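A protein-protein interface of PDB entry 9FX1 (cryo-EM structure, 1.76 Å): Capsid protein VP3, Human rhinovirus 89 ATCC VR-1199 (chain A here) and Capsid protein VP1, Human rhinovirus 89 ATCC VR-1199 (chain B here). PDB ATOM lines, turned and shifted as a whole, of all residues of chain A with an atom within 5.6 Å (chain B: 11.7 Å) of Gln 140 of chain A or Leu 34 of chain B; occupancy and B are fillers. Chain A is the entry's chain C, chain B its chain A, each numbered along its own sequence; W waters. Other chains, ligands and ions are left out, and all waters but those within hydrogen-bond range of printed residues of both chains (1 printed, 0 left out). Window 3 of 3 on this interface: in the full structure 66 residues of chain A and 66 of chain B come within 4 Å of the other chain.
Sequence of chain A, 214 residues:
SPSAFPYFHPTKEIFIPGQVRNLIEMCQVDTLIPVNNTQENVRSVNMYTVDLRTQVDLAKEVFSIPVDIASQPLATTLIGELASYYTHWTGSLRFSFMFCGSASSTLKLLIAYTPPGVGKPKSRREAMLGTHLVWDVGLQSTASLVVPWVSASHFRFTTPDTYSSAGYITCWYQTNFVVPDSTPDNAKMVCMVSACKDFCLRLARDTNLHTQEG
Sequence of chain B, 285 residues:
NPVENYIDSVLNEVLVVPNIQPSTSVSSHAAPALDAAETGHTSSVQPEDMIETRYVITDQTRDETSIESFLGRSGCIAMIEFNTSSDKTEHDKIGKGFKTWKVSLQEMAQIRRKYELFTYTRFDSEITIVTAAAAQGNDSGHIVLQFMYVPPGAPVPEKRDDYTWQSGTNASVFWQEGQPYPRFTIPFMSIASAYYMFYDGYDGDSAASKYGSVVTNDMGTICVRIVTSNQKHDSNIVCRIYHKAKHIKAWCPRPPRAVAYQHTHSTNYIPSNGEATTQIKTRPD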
ATOM      1  N   TRP A 135     -15.268 -30.942   7.647  1.00  0.00           N
ATOM      2  CA  TRP A 135     -15.088 -29.601   7.111  1.00  0.00           C
ATOM      3  C   TRP A 135     -16.157 -28.677   7.680  1.00  0.00           C
ATOM      4  O   TRP A 135     -17.344 -28.902   7.466  1.00  0.00           O
ATOM      5  CB  TRP A 135     -15.205 -29.673   5.587  1.00  0.00           C
ATOM      6  CG  TRP A 135     -15.272 -28.375   4.846  1.00  0.00           C
ATOM      7  CD1 TRP A 135     -14.794 -27.169   5.238  1.00  0.00           C
ATOM      8  CD2 TRP A 135     -15.830 -28.163   3.521  1.00  0.00           C
ATOM      9  NE1 TRP A 135     -15.024 -26.234   4.248  1.00  0.00           N
ATOM     10  CE2 TRP A 135     -15.640 -26.799   3.153  1.00  0.00           C
ATOM     11  CE3 TRP A 135     -16.457 -29.005   2.588  1.00  0.00           C
ATOM     12  CZ2 TRP A 135     -16.044 -26.303   1.907  1.00  0.00           C
ATOM     13  CZ3 TRP A 135     -16.870 -28.518   1.337  1.00  0.00           C
ATOM     14  CH2 TRP A 135     -16.661 -27.174   0.994  1.00  0.00           C
ATOM     15  N   ASP A 136     -15.732 -27.627   8.374  1.00  0.00           N
ATOM     16  CA  ASP A 136     -16.603 -26.535   8.803  1.00  0.00           C
ATOM     17  C   ASP A 136     -16.576 -25.406   7.770  1.00  0.00           C
ATOM     18  O   ASP A 136     -15.527 -24.807   7.536  1.00  0.00           O
ATOM     19  CB  ASP A 136     -16.113 -26.022  10.166  1.00  0.00           C
ATOM     20  CG  ASP A 136     -17.056 -24.969  10.754  1.00  0.00           C
ATOM     21  OD1 ASP A 136     -18.287 -25.153  10.637  1.00  0.00           O
ATOM     22  OD2 ASP A 136     -16.581 -24.034  11.427  1.00  0.00           O
ATOM     23  N   VAL A 137     -17.716 -25.102   7.155  1.00  0.00           N
ATOM     24  CA  VAL A 137     -17.824 -24.003   6.189  1.00  0.00           C
ATOM     25  C   VAL A 137     -17.816 -22.661   6.924  1.00  0.00           C
ATOM     26  O   VAL A 137     -18.682 -22.412   7.764  1.00  0.00           O
ATOM     27  CB  VAL A 137     -19.085 -24.179   5.330  1.00  0.00           C
ATOM     28  CG1 VAL A 137     -19.358 -22.989   4.424  1.00  0.00           C
ATOM     29  CG2 VAL A 137     -18.954 -25.418   4.437  1.00  0.00           C
ATOM     30  N   GLY A 138     -16.877 -21.775   6.593  1.00  0.00           N
ATOM     31  CA  GLY A 138     -16.685 -20.492   7.280  1.00  0.00           C
ATOM     32  C   GLY A 138     -16.105 -19.409   6.370  1.00  0.00           C
ATOM     33  O   GLY A 138     -16.357 -19.411   5.164  1.00  0.00           O
ATOM     34  N   LEU A 139     -15.327 -18.477   6.928  1.00  0.00           N
ATOM     35  CA  LEU A 139     -14.664 -17.430   6.142  1.00  0.00           C
ATOM     36  C   LEU A 139     -13.722 -18.001   5.067  1.00  0.00           C
ATOM     37  O   LEU A 139     -13.665 -17.452   3.965  1.00  0.00           O
ATOM     38  CB  LEU A 139     -13.904 -16.462   7.065  1.00  0.00           C
ATOM     39  CG  LEU A 139     -14.787 -15.634   8.017  1.00  0.00           C
ATOM     40  CD1 LEU A 139     -13.902 -14.727   8.870  1.00  0.00           C
ATOM     41  CD2 LEU A 139     -15.790 -14.748   7.278  1.00  0.00           C
ATOM     42  N   GLN A 140     -13.017 -19.102   5.342  1.00  0.00           N
ATOM     43  CA  GLN A 140     -12.294 -19.854   4.311  1.00  0.00           C
ATOM     44  C   GLN A 140     -13.282 -20.785   3.599  1.00  0.00           C
ATOM     45  O   GLN A 140     -13.856 -21.683   4.211  1.00  0.00           O
ATOM     46  CB  GLN A 140     -11.118 -20.624   4.929  1.00  0.00           C
ATOM     47  CG  GLN A 140     -10.034 -19.655   5.428  1.00  0.00           C
ATOM     48  CD  GLN A 140      -8.878 -20.388   6.095  1.00  0.00           C
ATOM     49  OE1 GLN A 140      -9.025 -21.002   7.140  1.00  0.00           O
ATOM     50  NE2 GLN A 140      -7.690 -20.334   5.539  1.00  0.00           N
ATOM     51  N   SER A 141     -13.532 -20.548   2.314  1.00  0.00           N
ATOM     52  CA  SER A 141     -14.620 -21.225   1.604  1.00  0.00           C
ATOM     53  C   SER A 141     -14.223 -22.572   1.009  1.00  0.00           C
ATOM     54  O   SER A 141     -15.057 -23.235   0.400  1.00  0.00           O
ATOM     55  CB  SER A 141     -15.173 -20.320   0.508  1.00  0.00           C
ATOM     56  OG  SER A 141     -16.552 -20.557   0.401  1.00  0.00           O
ATOM     57  N   THR A 142     -12.950 -22.949   1.112  1.00  0.00           N
ATOM     58  CA  THR A 142     -12.405 -24.145   0.477  1.00  0.00           C
ATOM     59  C   THR A 142     -11.791 -25.065   1.517  1.00  0.00           C
ATOM     60  O   THR A 142     -11.088 -24.615   2.415  1.00  0.00           O
ATOM     61  CB  THR A 142     -11.376 -23.791  -0.603  1.00  0.00           C
ATOM     62  OG1 THR A 142     -11.956 -22.893  -1.521  1.00  0.00           O
ATOM     63  CG2 THR A 142     -10.872 -24.997  -1.395  1.00  0.00           C
ATOM     64  N   ALA A 143     -12.006 -26.361   1.362  1.00  0.00           N
ATOM     65  CA  ALA A 143     -11.319 -27.374   2.144  1.00  0.00           C
ATOM     66  C   ALA A 143     -10.721 -28.437   1.236  1.00  0.00           C
ATOM     67  O   ALA A 143     -11.228 -28.675   0.147  1.00  0.00           O
ATOM     68  CB  ALA A 143     -12.274 -27.983   3.153  1.00  0.00           C
ATOM     69  N   SER A 144      -9.670 -29.102   1.692  1.00  0.00           N
ATOM     70  CA  SER A 144      -9.008 -30.160   0.940  1.00  0.00           C
ATOM     71  C   SER A 144      -8.988 -31.454   1.740  1.00  0.00           C
ATOM     72  O   SER A 144      -8.571 -31.452   2.885  1.00  0.00           O
ATOM     73  CB  SER A 144      -7.588 -29.738   0.557  1.00  0.00           C
ATOM     74  OG  SER A 144      -7.584 -28.552  -0.216  1.00  0.00           O
ATOM     75  N   SER B  28      -4.173 -27.517  16.721  1.00  0.00           N
ATOM     76  CA  SER B  28      -3.598 -26.192  16.466  1.00  0.00           C
ATOM     77  C   SER B  28      -4.609 -25.230  15.839  1.00  0.00           C
ATOM     78  O   SER B  28      -5.562 -25.660  15.189  1.00  0.00           O
ATOM     79  CB  SER B  28      -2.374 -26.353  15.550  1.00  0.00           C
ATOM     80  OG  SER B  28      -1.725 -25.122  15.318  1.00  0.00           O
ATOM     81  N   HIS B  29      -4.376 -23.922  15.980  1.00  0.00           N
ATOM     82  CA  HIS B  29      -5.077 -22.898  15.195  1.00  0.00           C
ATOM     83  C   HIS B  29      -4.672 -22.899  13.717  1.00  0.00           C
ATOM     84  O   HIS B  29      -5.429 -22.413  12.879  1.00  0.00           O
ATOM     85  CB  HIS B  29      -4.808 -21.509  15.786  1.00  0.00           C
ATOM     86  CG  HIS B  29      -5.435 -21.321  17.138  1.00  0.00           C
ATOM     87  ND1 HIS B  29      -6.801 -21.436  17.412  1.00  0.00           N
ATOM     88  CD2 HIS B  29      -4.788 -20.940  18.274  1.00  0.00           C
ATOM     89  CE1 HIS B  29      -6.943 -21.128  18.712  1.00  0.00           C
ATOM     90  NE2 HIS B  29      -5.752 -20.827  19.253  1.00  0.00           N
ATOM     91  N   ALA B  30      -3.497 -23.433  13.379  1.00  0.00           N
ATOM     92  CA  ALA B  30      -3.128 -23.668  11.989  1.00  0.00           C
ATOM     93  C   ALA B  30      -4.037 -24.758  11.403  1.00  0.00           C
ATOM     94  O   ALA B  30      -4.116 -25.864  11.942  1.00  0.00           O
ATOM     95  CB  ALA B  30      -1.650 -24.059  11.906  1.00  0.00           C
ATOM     96  N   ALA B  31      -4.696 -24.460  10.290  1.00  0.00           N
ATOM     97  CA  ALA B  31      -5.632 -25.366   9.637  1.00  0.00           C
ATOM     98  C   ALA B  31      -5.231 -25.564   8.164  1.00  0.00           C
ATOM     99  O   ALA B  31      -5.902 -25.035   7.278  1.00  0.00           O
ATOM    100  CB  ALA B  31      -7.055 -24.819   9.829  1.00  0.00           C
ATOM    101  N   PRO B  32      -4.140 -26.303   7.873  1.00  0.00           N
ATOM    102  CA  PRO B  32      -3.707 -26.567   6.498  1.00  0.00           C
ATOM    103  C   PRO B  32      -4.809 -27.113   5.576  1.00  0.00           C
ATOM    104  O   PRO B  32      -4.768 -26.881   4.372  1.00  0.00           O
ATOM    105  CB  PRO B  32      -2.585 -27.604   6.616  1.00  0.00           C
ATOM    106  CG  PRO B  32      -2.015 -27.388   8.012  1.00  0.00           C
ATOM    107  CD  PRO B  32      -3.227 -26.935   8.820  1.00  0.00           C
ATOM    108  N   ALA B  33      -5.797 -27.826   6.127  1.00  0.00           N
ATOM    109  CA  ALA B  33      -6.913 -28.371   5.356  1.00  0.00           C
ATOM    110  C   ALA B  33      -7.846 -27.295   4.768  1.00  0.00           C
ATOM    111  O   ALA B  33      -8.596 -27.597   3.847  1.00  0.00           O
ATOM    112  CB  ALA B  33      -7.717 -29.309   6.260  1.00  0.00           C
ATOM    113  N   LEU B  34      -7.839 -26.064   5.291  1.00  0.00           N
ATOM    114  CA  LEU B  34      -8.710 -24.967   4.866  1.00  0.00           C
ATOM    115  C   LEU B  34      -7.933 -23.937   4.039  1.00  0.00           C
ATOM    116  O   LEU B  34      -6.792 -23.602   4.347  1.00  0.00           O
ATOM    117  CB  LEU B  34      -9.365 -24.294   6.082  1.00  0.00           C
ATOM    118  CG  LEU B  34     -10.198 -25.228   6.977  1.00  0.00           C
ATOM    119  CD1 LEU B  34     -10.844 -24.413   8.095  1.00  0.00           C
ATOM    120  CD2 LEU B  34     -11.307 -25.942   6.209  1.00  0.00           C
ATOM    121  N   ASP B  35      -8.555 -23.419   2.986  1.00  0.00           N
ATOM    122  CA  ASP B  35      -7.954 -22.434   2.086  1.00  0.00           C
ATOM    123  C   ASP B  35      -9.040 -21.605   1.363  1.00  0.00           C
ATOM    124  O   ASP B  35     -10.237 -21.747   1.622  1.00  0.00           O
ATOM    125  CB  ASP B  35      -7.035 -23.179   1.087  1.00  0.00           C
ATOM    126  CG  ASP B  35      -5.996 -22.275   0.405  1.00  0.00           C
ATOM    127  OD1 ASP B  35      -5.867 -21.088   0.791  1.00  0.00           O
ATOM    128  OD2 ASP B  35      -5.339 -22.747  -0.544  1.00  0.00           O
ATOM    129  N   ALA B  36      -8.631 -20.762   0.418  1.00  0.00           N
ATOM    130  CA  ALA B  36      -9.500 -20.018  -0.480  1.00  0.00           C
ATOM    131  C   ALA B  36      -9.086 -20.279  -1.937  1.00  0.00           C
ATOM    132  O   ALA B  36      -8.184 -19.624  -2.463  1.00  0.00           O
ATOM    133  CB  ALA B  36      -9.420 -18.541  -0.078  1.00  0.00           C
ATOM    134  N   ALA B  37      -9.740 -21.232  -2.613  1.00  0.00           N
ATOM    135  CA  ALA B  37      -9.508 -21.486  -4.037  1.00  0.00           C
ATOM    136  C   ALA B  37      -9.827 -20.258  -4.905  1.00  0.00           C
ATOM    137  O   ALA B  37      -9.302 -20.137  -6.007  1.00  0.00           O
ATOM    138  CB  ALA B  37     -10.335 -22.690  -4.498  1.00  0.00           C
ATOM    139  N   GLU B  38     -10.610 -19.298  -4.398  1.00  0.00           N
ATOM    140  CA  GLU B  38     -10.877 -18.016  -5.058  1.00  0.00           C
ATOM    141  C   GLU B  38      -9.603 -17.277  -5.460  1.00  0.00           C
ATOM    142  O   GLU B  38      -9.590 -16.598  -6.482  1.00  0.00           O
ATOM    143  CB  GLU B  38     -11.701 -17.090  -4.154  1.00  0.00           C
ATOM    144  CG  GLU B  38     -13.101 -17.631  -3.852  1.00  0.00           C
ATOM    145  CD  GLU B  38     -13.201 -18.512  -2.595  1.00  0.00           C
ATOM    146  OE1 GLU B  38     -12.164 -18.991  -2.076  1.00  0.00           O
ATOM    147  OE2 GLU B  38     -14.335 -18.661  -2.086  1.00  0.00           O
ATOM    148  N   THR B  39      -8.520 -17.467  -4.699  1.00  0.00           N
ATOM    149  CA  THR B  39      -7.212 -16.881  -4.986  1.00  0.00           C
ATOM    150  C   THR B  39      -6.628 -17.323  -6.324  1.00  0.00           C
ATOM    151  O   THR B  39      -5.723 -16.660  -6.816  1.00  0.00           O
ATOM    152  CB  THR B  39      -6.184 -17.236  -3.900  1.00  0.00           C
ATOM    153  OG1 THR B  39      -5.981 -18.630  -3.860  1.00  0.00           O
ATOM    154  CG2 THR B  39      -6.565 -16.756  -2.502  1.00  0.00           C
ATOM    155  N   HIS B  41      -4.838 -19.965  -6.657  1.00  0.00           N
ATOM    156  CA  HIS B  41      -3.733 -20.839  -6.262  1.00  0.00           C
ATOM    157  C   HIS B  41      -4.281 -22.173  -5.756  1.00  0.00           C
ATOM    158  O   HIS B  41      -5.313 -22.229  -5.089  1.00  0.00           O
ATOM    159  CB  HIS B  41      -2.851 -20.138  -5.220  1.00  0.00           C
ATOM    160  CG  HIS B  41      -2.308 -18.830  -5.736  1.00  0.00           C
ATOM    161  ND1 HIS B  41      -1.523 -18.682  -6.884  1.00  0.00           N
ATOM    162  CD2 HIS B  41      -2.541 -17.599  -5.201  1.00  0.00           C
ATOM    163  CE1 HIS B  41      -1.307 -17.362  -7.014  1.00  0.00           C
ATOM    164  NE2 HIS B  41      -1.911 -16.689  -6.019  1.00  0.00           N
ATOM    165  N   THR B  42      -3.603 -23.263  -6.091  1.00  0.00           N
ATOM    166  CA  THR B  42      -3.955 -24.596  -5.589  1.00  0.00           C
ATOM    167  C   THR B  42      -3.436 -24.751  -4.158  1.00  0.00           C
ATOM    168  O   THR B  42      -2.316 -24.323  -3.876  1.00  0.00           O
ATOM    169  CB  THR B  42      -3.389 -25.661  -6.538  1.00  0.00           C
ATOM    170  OG1 THR B  42      -4.022 -25.529  -7.801  1.00  0.00           O
ATOM    171  CG2 THR B  42      -3.642 -27.071  -6.025  1.00  0.00           C
ATOM    172  N   SER B  43      -4.212 -25.352  -3.252  1.00  0.00           N
ATOM    173  CA  SER B  43      -3.787 -25.522  -1.856  1.00  0.00           C
ATOM    174  C   SER B  43      -2.441 -26.251  -1.760  1.00  0.00           C
ATOM    175  O   SER B  43      -2.195 -27.229  -2.462  1.00  0.00           O
ATOM    176  CB  SER B  43      -4.851 -26.264  -1.040  1.00  0.00           C
ATOM    177  OG  SER B  43      -4.342 -26.625   0.233  1.00  0.00           O
ATOM    178  N   SER B  44      -1.570 -25.779  -0.874  1.00  0.00           N
ATOM    179  CA  SER B  44      -0.248 -26.354  -0.623  1.00  0.00           C
ATOM    180  C   SER B  44      -0.283 -27.570   0.318  1.00  0.00           C
ATOM    181  O   SER B  44       0.770 -28.138   0.592  1.00  0.00           O
ATOM    182  CB  SER B  44       0.676 -25.265  -0.065  1.00  0.00           C
ATOM    183  OG  SER B  44       0.165 -24.768   1.156  1.00  0.00           O
ATOM    184  N   VAL B  45      -1.455 -27.982   0.820  1.00  0.00           N
ATOM    185  CA  VAL B  45      -1.560 -29.072   1.805  1.00  0.00           C
ATOM    186  C   VAL B  45      -1.008 -30.392   1.262  1.00  0.00           C
ATOM    187  O   VAL B  45      -1.237 -30.738   0.100  1.00  0.00           O
ATOM    188  CB  VAL B  45      -2.997 -29.217   2.339  1.00  0.00           C
ATOM    189  CG1 VAL B  45      -3.971 -29.878   1.365  1.00  0.00           C
ATOM    190  CG2 VAL B  45      -3.031 -30.029   3.632  1.00  0.00           C
ATOM    191  N   GLN B  46      -0.299 -31.138   2.101  1.00  0.00           N
ATOM    192  CA  GLN B  46       0.348 -32.416   1.773  1.00  0.00           C
ATOM    193  C   GLN B  46      -0.107 -33.502   2.766  1.00  0.00           C
ATOM    194  O   GLN B  46      -0.676 -33.168   3.806  1.00  0.00           O
ATOM    195  CB  GLN B  46       1.877 -32.227   1.806  1.00  0.00           C
ATOM    196  CG  GLN B  46       2.418 -31.176   0.822  1.00  0.00           C
ATOM    197  CD  GLN B  46       2.157 -31.471  -0.653  1.00  0.00           C
ATOM    198  OE1 GLN B  46       1.850 -32.584  -1.065  1.00  0.00           O
ATOM    199  NE2 GLN B  46       2.314 -30.500  -1.525  1.00  0.00           N
ATOM    200  N   ASP B  49       0.205 -33.212   6.668  1.00  0.00           N
ATOM    201  CA  ASP B  49      -0.626 -32.185   7.308  1.00  0.00           C
ATOM    202  C   ASP B  49      -2.020 -32.691   7.727  1.00  0.00           C
ATOM    203  O   ASP B  49      -2.696 -32.028   8.510  1.00  0.00           O
ATOM    204  CB  ASP B  49      -0.805 -31.010   6.337  1.00  0.00           C
ATOM    205  CG  ASP B  49       0.505 -30.395   5.835  1.00  0.00           C
ATOM    206  OD1 ASP B  49       1.441 -30.233   6.649  1.00  0.00           O
ATOM    207  OD2 ASP B  49       0.580 -30.028   4.640  1.00  0.00           O
ATOM    208  N   MET B  50      -2.477 -33.828   7.187  1.00  0.00           N
ATOM    209  CA  MET B  50      -3.875 -34.270   7.300  1.00  0.00           C
ATOM    210  C   MET B  50      -4.092 -35.717   7.747  1.00  0.00           C
ATOM    211  O   MET B  50      -5.208 -36.081   8.122  1.00  0.00           O
ATOM    212  CB  MET B  50      -4.586 -34.023   5.968  1.00  0.00           C
ATOM    213  CG  MET B  50      -4.782 -32.517   5.782  1.00  0.00           C
ATOM    214  SD  MET B  50      -6.115 -32.092   4.667  1.00  0.00           S
ATOM    215  CE  MET B  50      -7.526 -32.776   5.579  1.00  0.00           C
HETATM  216  O   HOH W   1     -12.607 -18.520   0.501  1.00  0.00           O
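The backbone NH (N) of Asp 35 of chain B is in hydrogen-bond range of the backbone carbonyl oxygen (O) of Thr 142 of chain A, at 2.9 Å.
O of Ala 33 of chain B lies within hydrogen-bond range of N of Ser 144 of chain A, at 2.8 Å.
The backbone carbonyl oxygen (O) of Ser 144 of chain A lies close to the side-chain sulfur (SD) of Met 50 of chain B (3.1 Å).
The side-chain hydroxyl (OG1) of Thr 142 of chain A sits at hydrogen-bond distance from the backbone NH (N) of Ala 37 of chain B (3.0 Å).
O of Ala 36 of chain B sits at hydrogen-bond distance from OG1 of Thr 39 of chain B, 2.8 Å away.
The side-chain hydroxyl (OG) of Ser 43 of chain B sits at hydrogen-bond distance from the backbone NH (N) of Val 45 of chain B, at 3.2 Å.
Among the printed residues, merely in contact across the chains: Trp 135 of chain A with Leu 34 of chain B (3.8 Å), Gln 140 of chain A with Leu 34 of chain B (3.5 Å), Gln 140 of chain A with Asp 35 of chain B (3.6 Å), Ser 141 of chain A with Asp 35 of chain B (3.6 Å), Ser 141 of chain A with Glu 38 of chain B (3.2 Å), Thr 142 of chain A with Leu 34 of chain B (3.4 Å), Thr 142 of chain A with Ala 36 of chain B (3.9 Å), Thr 142 of chain A with Glu 38 of chain B (3.9 Å), Ala 143 of chain A with Ala 33 of chain B (3.2 Å), Ala 143 of chain A with Leu 34 of chain B (3.8 Å), Ser 144 of chain A with Ser 43 of chain B (3.7 Å) and Ser 144 of chain A with Val 45 of chain B (3.7 Å).
Of the printed residues of chain B, Gln 140 of chain A touches Leu 34 (3.5 Å) and Asp 35 (3.6 Å).
Of chain A, only Trp 135, Gln 140, Thr 142 and Ala 143 come within 4 Å of Leu 34 of chain B.
No residue of chain B comes within 4 Å of Val 137 of chain A.
Ser 141 of chain A touches two residues of chain B.
Ala 143 of chain A touches just these residues of chain B: Ala 33 and Leu 34.
Printed residues of chain B within 4 Å of Trp 135 of chain A: Leu 34 (3.8 Å).
Of the printed residues of chain A, Ala 36 of chain B touches Thr 142 (3.9 Å).
Printed residues of chain A within 4 Å of Ala 37 of chain B: Thr 142 (3.0 Å).
Of the printed residues of chain A, Val 45 of chain B touches Ser 144.
Printed residues of chain A within 4 Å of Asp 35 of chain B: Gln 140 (3.6 Å), Ser 141 (3.6 Å) and Thr 142 (2.9 Å).
His 41 of chain B touches none of the printed residues of chain A.
The nearest residue of chain A that does not touch Leu 34 of chain B is Asp 136 of chain A (4.6 Å).
The nearest printed residue of chain A that does not touch Asp 35 of chain B is Ala 143 of chain A (4.8 Å).
Hydrophobic or aromatic side chains of chain B within 4 Å of the printed part of chain A: Leu 34, Ala 37, Val 45 and Met 50.
Among the printed residues, 16 pairs touch across the chains.
Among the printed residues, no Asp or Glu carboxylate lies within 4 Å of a Lys or Arg side-chain nitrogen of the other chain.
Water W1 bridges OE1 of Glu 38 of chain B and N of Ser 141 of chain A.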
